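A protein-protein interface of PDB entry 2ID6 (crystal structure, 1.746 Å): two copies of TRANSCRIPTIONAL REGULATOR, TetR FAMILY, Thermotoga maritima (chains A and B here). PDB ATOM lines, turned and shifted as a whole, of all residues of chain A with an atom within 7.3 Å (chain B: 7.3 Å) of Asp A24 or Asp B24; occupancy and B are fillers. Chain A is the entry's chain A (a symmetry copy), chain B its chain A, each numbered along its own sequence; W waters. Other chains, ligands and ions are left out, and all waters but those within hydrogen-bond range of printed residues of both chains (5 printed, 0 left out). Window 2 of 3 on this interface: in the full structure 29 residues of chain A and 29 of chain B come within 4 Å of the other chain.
Of the printed residues of chain B, Arg A25 touches Asp B24 (2.9 Å), Ser B110 (2.9 Å), Val B111 (3.3 Å) and Asp B112 (3.2 Å). Of the printed residues of chain B, Val A111 touches Arg B25 (3.3 Å). Of the printed residues of chain B, Asp A112 touches Arg B25 (3.2 Å). Of the printed residues of chain A, Asp B24 touches Asp A24 and Arg A25. Printed residues of chain A within 4 Å of Arg B25: Asp A24, Ser A110, Val A111 and Asp A112. Of the printed residues of chain A, Asp B112 touches Arg A25. The nearest printed residue of chain B that does not touch Asp A112 is Lys B21 (6.6 Å).
Water W4 bridges the side-chain carboxylate (OD1) of Asp A112 and the guanidinium group (NE) of Arg B25. Water W3 lies within hydrogen-bond range of the side-chain carboxylate of Asp B112 (2.7 Å) and the guanidinium group of Arg A25 (3.2 Å). Water W2 lies within hydrogen-bond range of the backbone carbonyl oxygen of Lys B21 (2.7 Å), the backbone NH of Arg B25 (2.8 Å), the backbone NH of Asp B24 (3.2 Å) and the side-chain carboxylate of Asp A24 (3.3 Å). Water W5 lies within hydrogen-bond range of the backbone carbonyl oxygen (O) of Lys A21 (2.7 Å), the backbone NH (N) of Arg A25 (2.8 Å), the backbone NH (N) of Asp A24 (3.2 Å) and the side-chain carboxylate (OD2) of Asp B24 (3.3 Å). Water W1 lies within hydrogen-bond range of N of Ser A110 (3.1 Å) and N of Ser B110 (3.1 Å).
The guanidinium group (NE) of Arg A25 lies within salt-bridge range of the side-chain carboxylate (OD1) of Asp B24, at 2.9 Å. NE of Arg B25 is in salt-bridge range of OD1 of Asp A24 (2.9 Å). The backbone carbonyl oxygen (O) of Ser A110 is in hydrogen-bond range of the guanidinium group (NH2) of Arg B25 (2.9 Å). The backbone carbonyl oxygen of Ser B110 is in hydrogen-bond range of the guanidinium group of Arg A25, 2.9 Å away. The guanidinium group of Arg A25 sits close to the backbone NH of Asp B112, 3.2 Å away. The backbone NH of Asp A112 sits close to the guanidinium group of Arg B25 (3.2 Å).
O of Lys B21 is in hydrogen-bond range of NH1 of Arg B25, at 3.1 Å. The side-chain amino group (NZ) of Lys B49 lies within hydrogen-bond range of the backbone carbonyl oxygen (O) of Asp B24 (3.1 Å). The guanidinium group (NH1) of Arg A25 lies within hydrogen-bond range of the backbone carbonyl oxygen (O) of Lys A21, at 3.1 Å. O of Asp A24 lies within hydrogen-bond range of NZ of Lys A49 (3.1 Å).
Asp A24 touches Asp B24 (CB to CB, 3.6 Å). C of Val B111 touches NH2 of Arg A25 (3.3 Å). Val A111 touches Arg B25 (C to NH2, 3.3 Å).
Asp B24 touches its own counterpart, Asp A24. Asp A24 touches Arg B25, and with the chains exchanged Arg A25 touches Asp B24. Arg A25 touches Ser B110, and with the chains exchanged Ser A110 touches Arg B25. Arg A25 touches Val B111, and with the chains exchanged Val A111 touches Arg B25.
Printed residues of chain B that touch a printed residue of chain A: Asp B24, Arg B25, Ser B110, Val B111 and Asp B112. Among the printed residues, 9 pairs touch across the chains.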
ATOM      1  N   PHE A  18     -27.988  23.981 -36.414  1.00  0.00           N
ATOM      2  CA  PHE A  18     -26.959  23.278 -35.626  1.00  0.00           C
ATOM      3  C   PHE A  18     -26.065  24.254 -34.835  1.00  0.00           C
ATOM      4  O   PHE A  18     -25.710  23.970 -33.692  1.00  0.00           O
ATOM      5  CB  PHE A  18     -26.073  22.417 -36.513  1.00  0.00           C
ATOM      6  CG  PHE A  18     -26.734  21.174 -37.078  1.00  0.00           C
ATOM      7  CD1 PHE A  18     -27.463  20.310 -36.265  1.00  0.00           C
ATOM      8  CD2 PHE A  18     -26.493  20.810 -38.410  1.00  0.00           C
ATOM      9  CE1 PHE A  18     -28.020  19.129 -36.790  1.00  0.00           C
ATOM     10  CE2 PHE A  18     -27.038  19.637 -38.951  1.00  0.00           C
ATOM     11  CZ  PHE A  18     -27.821  18.791 -38.101  1.00  0.00           C
ATOM     12  N   LYS A  21     -28.367  25.481 -31.830  1.00  0.00           N
ATOM     13  CA  LYS A  21     -28.960  24.525 -30.902  1.00  0.00           C
ATOM     14  C   LYS A  21     -28.071  23.341 -30.558  1.00  0.00           C
ATOM     15  O   LYS A  21     -28.353  22.607 -29.614  1.00  0.00           O
ATOM     16  CB  LYS A  21     -30.314  24.048 -31.437  1.00  0.00           C
ATOM     17  CG  LYS A  21     -31.285  25.205 -31.670  1.00  0.00           C
ATOM     18  CD  LYS A  21     -32.718  24.749 -31.721  1.00  0.00           C
ATOM     19  CE  LYS A  21     -33.650  25.930 -31.890  1.00  0.00           C
ATOM     20  NZ  LYS A  21     -35.049  25.474 -31.717  1.00  0.00           N
ATOM     21  N   GLY A  22     -26.990  23.169 -31.311  1.00  0.00           N
ATOM     22  CA  GLY A  22     -26.184  21.962 -31.191  1.00  0.00           C
ATOM     23  C   GLY A  22     -26.819  20.826 -31.987  1.00  0.00           C
ATOM     24  O   GLY A  22     -27.960  20.945 -32.450  1.00  0.00           O
ATOM     25  N   TYR A  23     -26.076  19.720 -32.125  1.00  0.00           N
ATOM     26  CA  TYR A  23     -26.505  18.584 -32.931  1.00  0.00           C
ATOM     27  C   TYR A  23     -27.720  17.877 -32.349  1.00  0.00           C
ATOM     28  O   TYR A  23     -28.680  17.594 -33.058  1.00  0.00           O
ATOM     29  CB  TYR A  23     -25.359  17.588 -33.014  1.00  0.00           C
ATOM     30  CG  TYR A  23     -25.682  16.311 -33.736  1.00  0.00           C
ATOM     31  CD1 TYR A  23     -26.021  16.318 -35.079  1.00  0.00           C
ATOM     32  CD2 TYR A  23     -25.595  15.093 -33.079  1.00  0.00           C
ATOM     33  CE1 TYR A  23     -26.302  15.153 -35.748  1.00  0.00           C
ATOM     34  CE2 TYR A  23     -25.872  13.900 -33.735  1.00  0.00           C
ATOM     35  CZ  TYR A  23     -26.232  13.948 -35.077  1.00  0.00           C
ATOM     36  OH  TYR A  23     -26.503  12.777 -35.742  1.00  0.00           O
ATOM     37  N   ASP A  24     -27.638  17.556 -31.067  1.00  0.00           N
ATOM     38  CA  ASP A  24     -28.683  16.768 -30.416  1.00  0.00           C
ATOM     39  C   ASP A  24     -30.030  17.457 -30.403  1.00  0.00           C
ATOM     40  O   ASP A  24     -31.017  16.837 -30.777  1.00  0.00           O
ATOM     41  CB  ASP A  24     -28.265  16.350 -29.001  1.00  0.00           C
ATOM     42  CG  ASP A  24     -27.065  15.445 -28.988  1.00  0.00           C
ATOM     43  OD1 ASP A  24     -26.962  14.513 -29.825  1.00  0.00           O
ATOM     44  OD2 ASP A  24     -26.190  15.669 -28.114  1.00  0.00           O
ATOM     45  N   ARG A  25     -30.059  18.718 -29.974  1.00  0.00           N
ATOM     46  CA  ARG A  25     -31.284  19.487 -29.856  1.00  0.00           C
ATOM     47  C   ARG A  25     -31.898  19.842 -31.217  1.00  0.00           C
ATOM     48  O   ARG A  25     -33.123  19.813 -31.365  1.00  0.00           O
ATOM     49  CB  ARG A  25     -31.066  20.736 -28.989  1.00  0.00           C
ATOM     50  CG  ARG A  25     -31.335  20.500 -27.502  1.00  0.00           C
ATOM     51  CD  ARG A  25     -30.864  21.643 -26.598  1.00  0.00           C
ATOM     52  NE  ARG A  25     -29.579  21.329 -25.971  1.00  0.00           N
ATOM     53  CZ  ARG A  25     -28.503  22.112 -26.000  1.00  0.00           C
ATOM     54  NH1 ARG A  25     -28.547  23.293 -26.604  1.00  0.00           N
ATOM     55  NH2 ARG A  25     -27.381  21.715 -25.404  1.00  0.00           N
ATOM     56  N   ALA A  26     -31.050  20.121 -32.212  1.00  0.00           N
ATOM     57  CA  ALA A  26     -31.542  20.521 -33.543  1.00  0.00           C
ATOM     58  C   ALA A  26     -32.473  19.451 -34.094  1.00  0.00           C
ATOM     59  O   ALA A  26     -32.260  18.251 -33.879  1.00  0.00           O
ATOM     60  CB  ALA A  26     -30.381  20.759 -34.505  1.00  0.00           C
ATOM     61  N   THR A  27     -33.520  19.876 -34.796  1.00  0.00           N
ATOM     62  CA  THR A  27     -34.423  18.933 -35.438  1.00  0.00           C
ATOM     63  C   THR A  27     -34.393  19.093 -36.948  1.00  0.00           C
ATOM     64  O   THR A  27     -34.297  20.220 -37.445  1.00  0.00           O
ATOM     65  CB  THR A  27     -35.890  19.135 -34.971  1.00  0.00           C
ATOM     66  OG1 THR A  27     -36.352  20.435 -35.381  1.00  0.00           O
ATOM     67  CG2 THR A  27     -36.000  19.010 -33.448  1.00  0.00           C
ATOM     68  N   LYS A  49     -30.396  12.877 -40.032  1.00  0.00           N
ATOM     69  CA  LYS A  49     -29.743  14.000 -39.356  1.00  0.00           C
ATOM     70  C   LYS A  49     -28.210  13.853 -39.251  1.00  0.00           C
ATOM     71  O   LYS A  49     -27.487  14.843 -39.360  1.00  0.00           O
ATOM     72  CB  LYS A  49     -30.380  14.266 -37.995  1.00  0.00           C
ATOM     73  CG  LYS A  49     -30.114  15.672 -37.440  1.00  0.00           C
ATOM     74  CD  LYS A  49     -30.786  15.953 -36.087  1.00  0.00           C
ATOM     75  CE  LYS A  49     -30.121  15.246 -34.928  1.00  0.00           C
ATOM     76  NZ  LYS A  49     -30.722  15.654 -33.618  1.00  0.00           N
ATOM     77  N   TYR A  53     -25.669  16.573 -40.903  1.00  0.00           N
ATOM     78  CA  TYR A  53     -24.601  17.240 -40.119  1.00  0.00           C
ATOM     79  C   TYR A  53     -23.237  16.993 -40.790  1.00  0.00           C
ATOM     80  O   TYR A  53     -22.412  17.924 -40.945  1.00  0.00           O
ATOM     81  CB  TYR A  53     -24.581  16.721 -38.676  1.00  0.00           C
ATOM     82  CG  TYR A  53     -23.572  17.480 -37.815  1.00  0.00           C
ATOM     83  CD1 TYR A  53     -23.961  18.575 -37.059  1.00  0.00           C
ATOM     84  CD2 TYR A  53     -22.234  17.075 -37.751  1.00  0.00           C
ATOM     85  CE1 TYR A  53     -23.035  19.261 -36.246  1.00  0.00           C
ATOM     86  CE2 TYR A  53     -21.301  17.760 -36.958  1.00  0.00           C
ATOM     87  CZ  TYR A  53     -21.704  18.845 -36.226  1.00  0.00           C
ATOM     88  OH  TYR A  53     -20.785  19.509 -35.447  1.00  0.00           O
ATOM     89  N   SER A 110     -19.925  18.366 -29.318  1.00  0.00           N
ATOM     90  CA  SER A 110     -21.269  17.943 -28.857  1.00  0.00           C
ATOM     91  C   SER A 110     -21.750  16.600 -29.412  1.00  0.00           C
ATOM     92  O   SER A 110     -22.445  15.880 -28.706  1.00  0.00           O
ATOM     93  CB  SER A 110     -22.338  19.067 -29.074  1.00  0.00           C
ATOM     94  OG  SER A 110     -22.953  19.175 -30.394  1.00  0.00           O
ATOM     95  N   VAL A 111     -21.357  16.255 -30.645  1.00  0.00           N
ATOM     96  CA  VAL A 111     -21.894  15.048 -31.317  1.00  0.00           C
ATOM     97  C   VAL A 111     -21.396  13.741 -30.664  1.00  0.00           C
ATOM     98  O   VAL A 111     -20.442  13.762 -29.899  1.00  0.00           O
ATOM     99  CB  VAL A 111     -21.648  15.072 -32.861  1.00  0.00           C
ATOM    100  CG1 VAL A 111     -22.018  16.447 -33.454  1.00  0.00           C
ATOM    101  CG2 VAL A 111     -20.233  14.735 -33.172  1.00  0.00           C
ATOM    102  N   ASP A 112     -22.065  12.618 -30.940  1.00  0.00           N
ATOM    103  CA  ASP A 112     -21.673  11.315 -30.373  1.00  0.00           C
ATOM    104  C   ASP A 112     -20.328  10.872 -30.939  1.00  0.00           C
ATOM    105  O   ASP A 112     -19.899  11.359 -31.995  1.00  0.00           O
ATOM    106  CB  ASP A 112     -22.706  10.274 -30.738  1.00  0.00           C
ATOM    107  CG  ASP A 112     -22.850  10.141 -32.225  1.00  0.00           C
ATOM    108  OD1 ASP A 112     -23.708  10.867 -32.780  1.00  0.00           O
ATOM    109  OD2 ASP A 112     -22.057   9.380 -32.844  1.00  0.00           O
ATOM    110  N   PHE B  18     -24.383  10.794 -17.625  1.00  0.00           N
ATOM    111  CA  PHE B  18     -23.988  12.043 -18.304  1.00  0.00           C
ATOM    112  C   PHE B  18     -22.577  11.949 -18.918  1.00  0.00           C
ATOM    113  O   PHE B  18     -22.351  12.456 -20.015  1.00  0.00           O
ATOM    114  CB  PHE B  18     -24.028  13.228 -17.352  1.00  0.00           C
ATOM    115  CG  PHE B  18     -25.416  13.686 -16.944  1.00  0.00           C
ATOM    116  CD1 PHE B  18     -26.417  13.886 -17.891  1.00  0.00           C
ATOM    117  CD2 PHE B  18     -25.659  14.049 -15.613  1.00  0.00           C
ATOM    118  CE1 PHE B  18     -27.682  14.370 -17.506  1.00  0.00           C
ATOM    119  CE2 PHE B  18     -26.911  14.533 -15.210  1.00  0.00           C
ATOM    120  CZ  PHE B  18     -27.935  14.687 -16.200  1.00  0.00           C
ATOM    121  N   LYS B  21     -23.051   9.659 -22.136  1.00  0.00           N
ATOM    122  CA  LYS B  21     -23.998  10.025 -23.182  1.00  0.00           C
ATOM    123  C   LYS B  21     -24.086  11.516 -23.466  1.00  0.00           C
ATOM    124  O   LYS B  21     -24.655  11.923 -24.475  1.00  0.00           O
ATOM    125  CB  LYS B  21     -25.382   9.453 -22.859  1.00  0.00           C
ATOM    126  CG  LYS B  21     -25.358   7.933 -22.699  1.00  0.00           C
ATOM    127  CD  LYS B  21     -26.721   7.318 -22.863  1.00  0.00           C
ATOM    128  CE  LYS B  21     -26.643   5.809 -22.760  1.00  0.00           C
ATOM    129  NZ  LYS B  21     -27.952   5.228 -23.142  1.00  0.00           N
ATOM    130  N   GLY B  22     -23.507  12.324 -22.584  1.00  0.00           N
ATOM    131  CA  GLY B  22     -23.701  13.766 -22.658  1.00  0.00           C
ATOM    132  C   GLY B  22     -25.029  14.149 -22.012  1.00  0.00           C
ATOM    133  O   GLY B  22     -25.851  13.279 -21.701  1.00  0.00           O
ATOM    134  N   TYR B  23     -25.237  15.460 -21.833  1.00  0.00           N
ATOM    135  CA  TYR B  23     -26.415  15.980 -21.151  1.00  0.00           C
ATOM    136  C   TYR B  23     -27.700  15.730 -21.925  1.00  0.00           C
ATOM    137  O   TYR B  23     -28.689  15.265 -21.367  1.00  0.00           O
ATOM    138  CB  TYR B  23     -26.246  17.481 -20.967  1.00  0.00           C
ATOM    139  CG  TYR B  23     -27.429  18.180 -20.361  1.00  0.00           C
ATOM    140  CD1 TYR B  23     -27.853  17.881 -19.077  1.00  0.00           C
ATOM    141  CD2 TYR B  23     -28.086  19.180 -21.062  1.00  0.00           C
ATOM    142  CE1 TYR B  23     -28.923  18.528 -18.511  1.00  0.00           C
ATOM    143  CE2 TYR B  23     -29.171  19.852 -20.511  1.00  0.00           C
ATOM    144  CZ  TYR B  23     -29.583  19.507 -19.228  1.00  0.00           C
ATOM    145  OH  TYR B  23     -30.650  20.166 -18.666  1.00  0.00           O
ATOM    146  N   ASP B  24     -27.682  16.089 -23.200  1.00  0.00           N
ATOM    147  CA  ASP B  24     -28.887  16.015 -24.024  1.00  0.00           C
ATOM    148  C   ASP B  24     -29.417  14.606 -24.182  1.00  0.00           C
ATOM    149  O   ASP B  24     -30.605  14.393 -23.975  1.00  0.00           O
ATOM    150  CB  ASP B  24     -28.668  16.677 -25.390  1.00  0.00           C
ATOM    151  CG  ASP B  24     -28.386  18.150 -25.289  1.00  0.00           C
ATOM    152  OD1 ASP B  24     -29.042  18.870 -24.495  1.00  0.00           O
ATOM    153  OD2 ASP B  24     -27.478  18.609 -26.025  1.00  0.00           O
ATOM    154  N   ARG B  25     -28.543  13.669 -24.546  1.00  0.00           N
ATOM    155  CA  ARG B  25     -28.916  12.287 -24.787  1.00  0.00           C
ATOM    156  C   ARG B  25     -29.314  11.545 -23.503  1.00  0.00           C
ATOM    157  O   ARG B  25     -30.253  10.745 -23.522  1.00  0.00           O
ATOM    158  CB  ARG B  25     -27.810  11.546 -25.551  1.00  0.00           C
ATOM    159  CG  ARG B  25     -27.966  11.620 -27.072  1.00  0.00           C
ATOM    160  CD  ARG B  25     -26.738  11.128 -27.844  1.00  0.00           C
ATOM    161  NE  ARG B  25     -25.919  12.247 -28.310  1.00  0.00           N
ATOM    162  CZ  ARG B  25     -24.611  12.378 -28.097  1.00  0.00           C
ATOM    163  NH1 ARG B  25     -23.940  11.437 -27.444  1.00  0.00           N
ATOM    164  NH2 ARG B  25     -23.971  13.450 -28.557  1.00  0.00           N
ATOM    165  N   ALA B  26     -28.638  11.850 -22.391  1.00  0.00           N
ATOM    166  CA  ALA B  26     -28.910  11.157 -21.120  1.00  0.00           C
ATOM    167  C   ALA B  26     -30.380  11.307 -20.753  1.00  0.00           C
ATOM    168  O   ALA B  26     -30.993  12.354 -20.999  1.00  0.00           O
ATOM    169  CB  ALA B  26     -28.028  11.703 -19.999  1.00  0.00           C
ATOM    170  N   THR B  27     -30.961  10.258 -20.177  1.00  0.00           N
ATOM    171  CA  THR B  27     -32.337  10.328 -19.710  1.00  0.00           C
ATOM    172  C   THR B  27     -32.411  10.151 -18.204  1.00  0.00           C
ATOM    173  O   THR B  27     -31.657   9.350 -17.641  1.00  0.00           O
ATOM    174  CB  THR B  27     -33.219   9.227 -20.358  1.00  0.00           C
ATOM    175  OG1 THR B  27     -32.749   7.929 -19.947  1.00  0.00           O
ATOM    176  CG2 THR B  27     -33.179   9.325 -21.886  1.00  0.00           C
ATOM    177  N   LYS B  49     -34.018  17.284 -14.936  1.00  0.00           N
ATOM    178  CA  LYS B  49     -32.701  16.916 -15.460  1.00  0.00           C
ATOM    179  C   LYS B  49     -31.657  18.049 -15.366  1.00  0.00           C
ATOM    180  O   LYS B  49     -30.483  17.787 -15.111  1.00  0.00           O
ATOM    181  CB  LYS B  49     -32.810  16.363 -16.878  1.00  0.00           C
ATOM    182  CG  LYS B  49     -31.606  15.520 -17.320  1.00  0.00           C
ATOM    183  CD  LYS B  49     -31.732  14.933 -18.734  1.00  0.00           C
ATOM    184  CE  LYS B  49     -31.558  15.962 -19.828  1.00  0.00           C
ATOM    185  NZ  LYS B  49     -31.554  15.326 -21.185  1.00  0.00           N
ATOM    186  N   TYR B  53     -28.202  17.627 -13.252  1.00  0.00           N
ATOM    187  CA  TYR B  53     -26.870  17.880 -13.852  1.00  0.00           C
ATOM    188  C   TYR B  53     -26.121  18.937 -13.018  1.00  0.00           C
ATOM    189  O   TYR B  53     -24.917  18.783 -12.707  1.00  0.00           O
ATOM    190  CB  TYR B  53     -27.007  18.354 -15.304  1.00  0.00           C
ATOM    191  CG  TYR B  53     -25.646  18.503 -15.981  1.00  0.00           C
ATOM    192  CD1 TYR B  53     -25.102  17.467 -16.726  1.00  0.00           C
ATOM    193  CD2 TYR B  53     -24.923  19.698 -15.887  1.00  0.00           C
ATOM    194  CE1 TYR B  53     -23.858  17.613 -17.372  1.00  0.00           C
ATOM    195  CE2 TYR B  53     -23.677  19.848 -16.512  1.00  0.00           C
ATOM    196  CZ  TYR B  53     -23.153  18.809 -17.234  1.00  0.00           C
ATOM    197  OH  TYR B  53     -21.932  18.965 -17.849  1.00  0.00           O
ATOM    198  N   SER B 110     -21.241  20.703 -23.859  1.00  0.00           N
ATOM    199  CA  SER B 110     -22.448  20.148 -24.516  1.00  0.00           C
ATOM    200  C   SER B 110     -23.768  20.800 -24.100  1.00  0.00           C
ATOM    201  O   SER B 110     -24.664  20.911 -24.928  1.00  0.00           O
ATOM    202  CB  SER B 110     -22.515  18.588 -24.387  1.00  0.00           C
ATOM    203  OG  SER B 110     -23.072  18.031 -23.157  1.00  0.00           O
ATOM    204  N   VAL B 111     -23.874  21.255 -22.845  1.00  0.00           N
ATOM    205  CA  VAL B 111     -25.161  21.764 -22.313  1.00  0.00           C
ATOM    206  C   VAL B 111     -25.577  23.103 -22.960  1.00  0.00           C
ATOM    207  O   VAL B 111     -24.759  23.760 -23.588  1.00  0.00           O
ATOM    208  CB  VAL B 111     -25.170  21.830 -20.751  1.00  0.00           C
ATOM    209  CG1 VAL B 111     -24.608  20.529 -20.144  1.00  0.00           C
ATOM    210  CG2 VAL B 111     -24.396  23.007 -20.271  1.00  0.00           C
ATOM    211  N   ASP B 112     -26.851  23.481 -22.834  1.00  0.00           N
ATOM    212  CA  ASP B 112     -27.354  24.742 -23.409  1.00  0.00           C
ATOM    213  C   ASP B 112     -26.736  25.937 -22.692  1.00  0.00           C
ATOM    214  O   ASP B 112     -26.238  25.805 -21.564  1.00  0.00           O
ATOM    215  CB  ASP B 112     -28.855  24.811 -23.239  1.00  0.00           C
ATOM    216  CG  ASP B 112     -29.247  24.739 -21.794  1.00  0.00           C
ATOM    217  OD1 ASP B 112     -29.470  23.599 -21.321  1.00  0.00           O
ATOM    218  OD2 ASP B 112     -29.253  25.802 -21.114  1.00  0.00           O
HETATM  219  O   HOH W   1     -20.242  19.665 -26.562  1.00  0.00           O
HETATM  220  O   HOH W   2     -25.855  14.295 -25.133  1.00  0.00           O
HETATM  221  O   HOH W   3     -30.558  21.778 -23.002  1.00  0.00           O
HETATM  222  O   HOH W   4     -25.943  11.415 -31.356  1.00  0.00           O
HETATM  223  O   HOH W   5     -27.746  20.009 -29.001  1.00  0.00           O
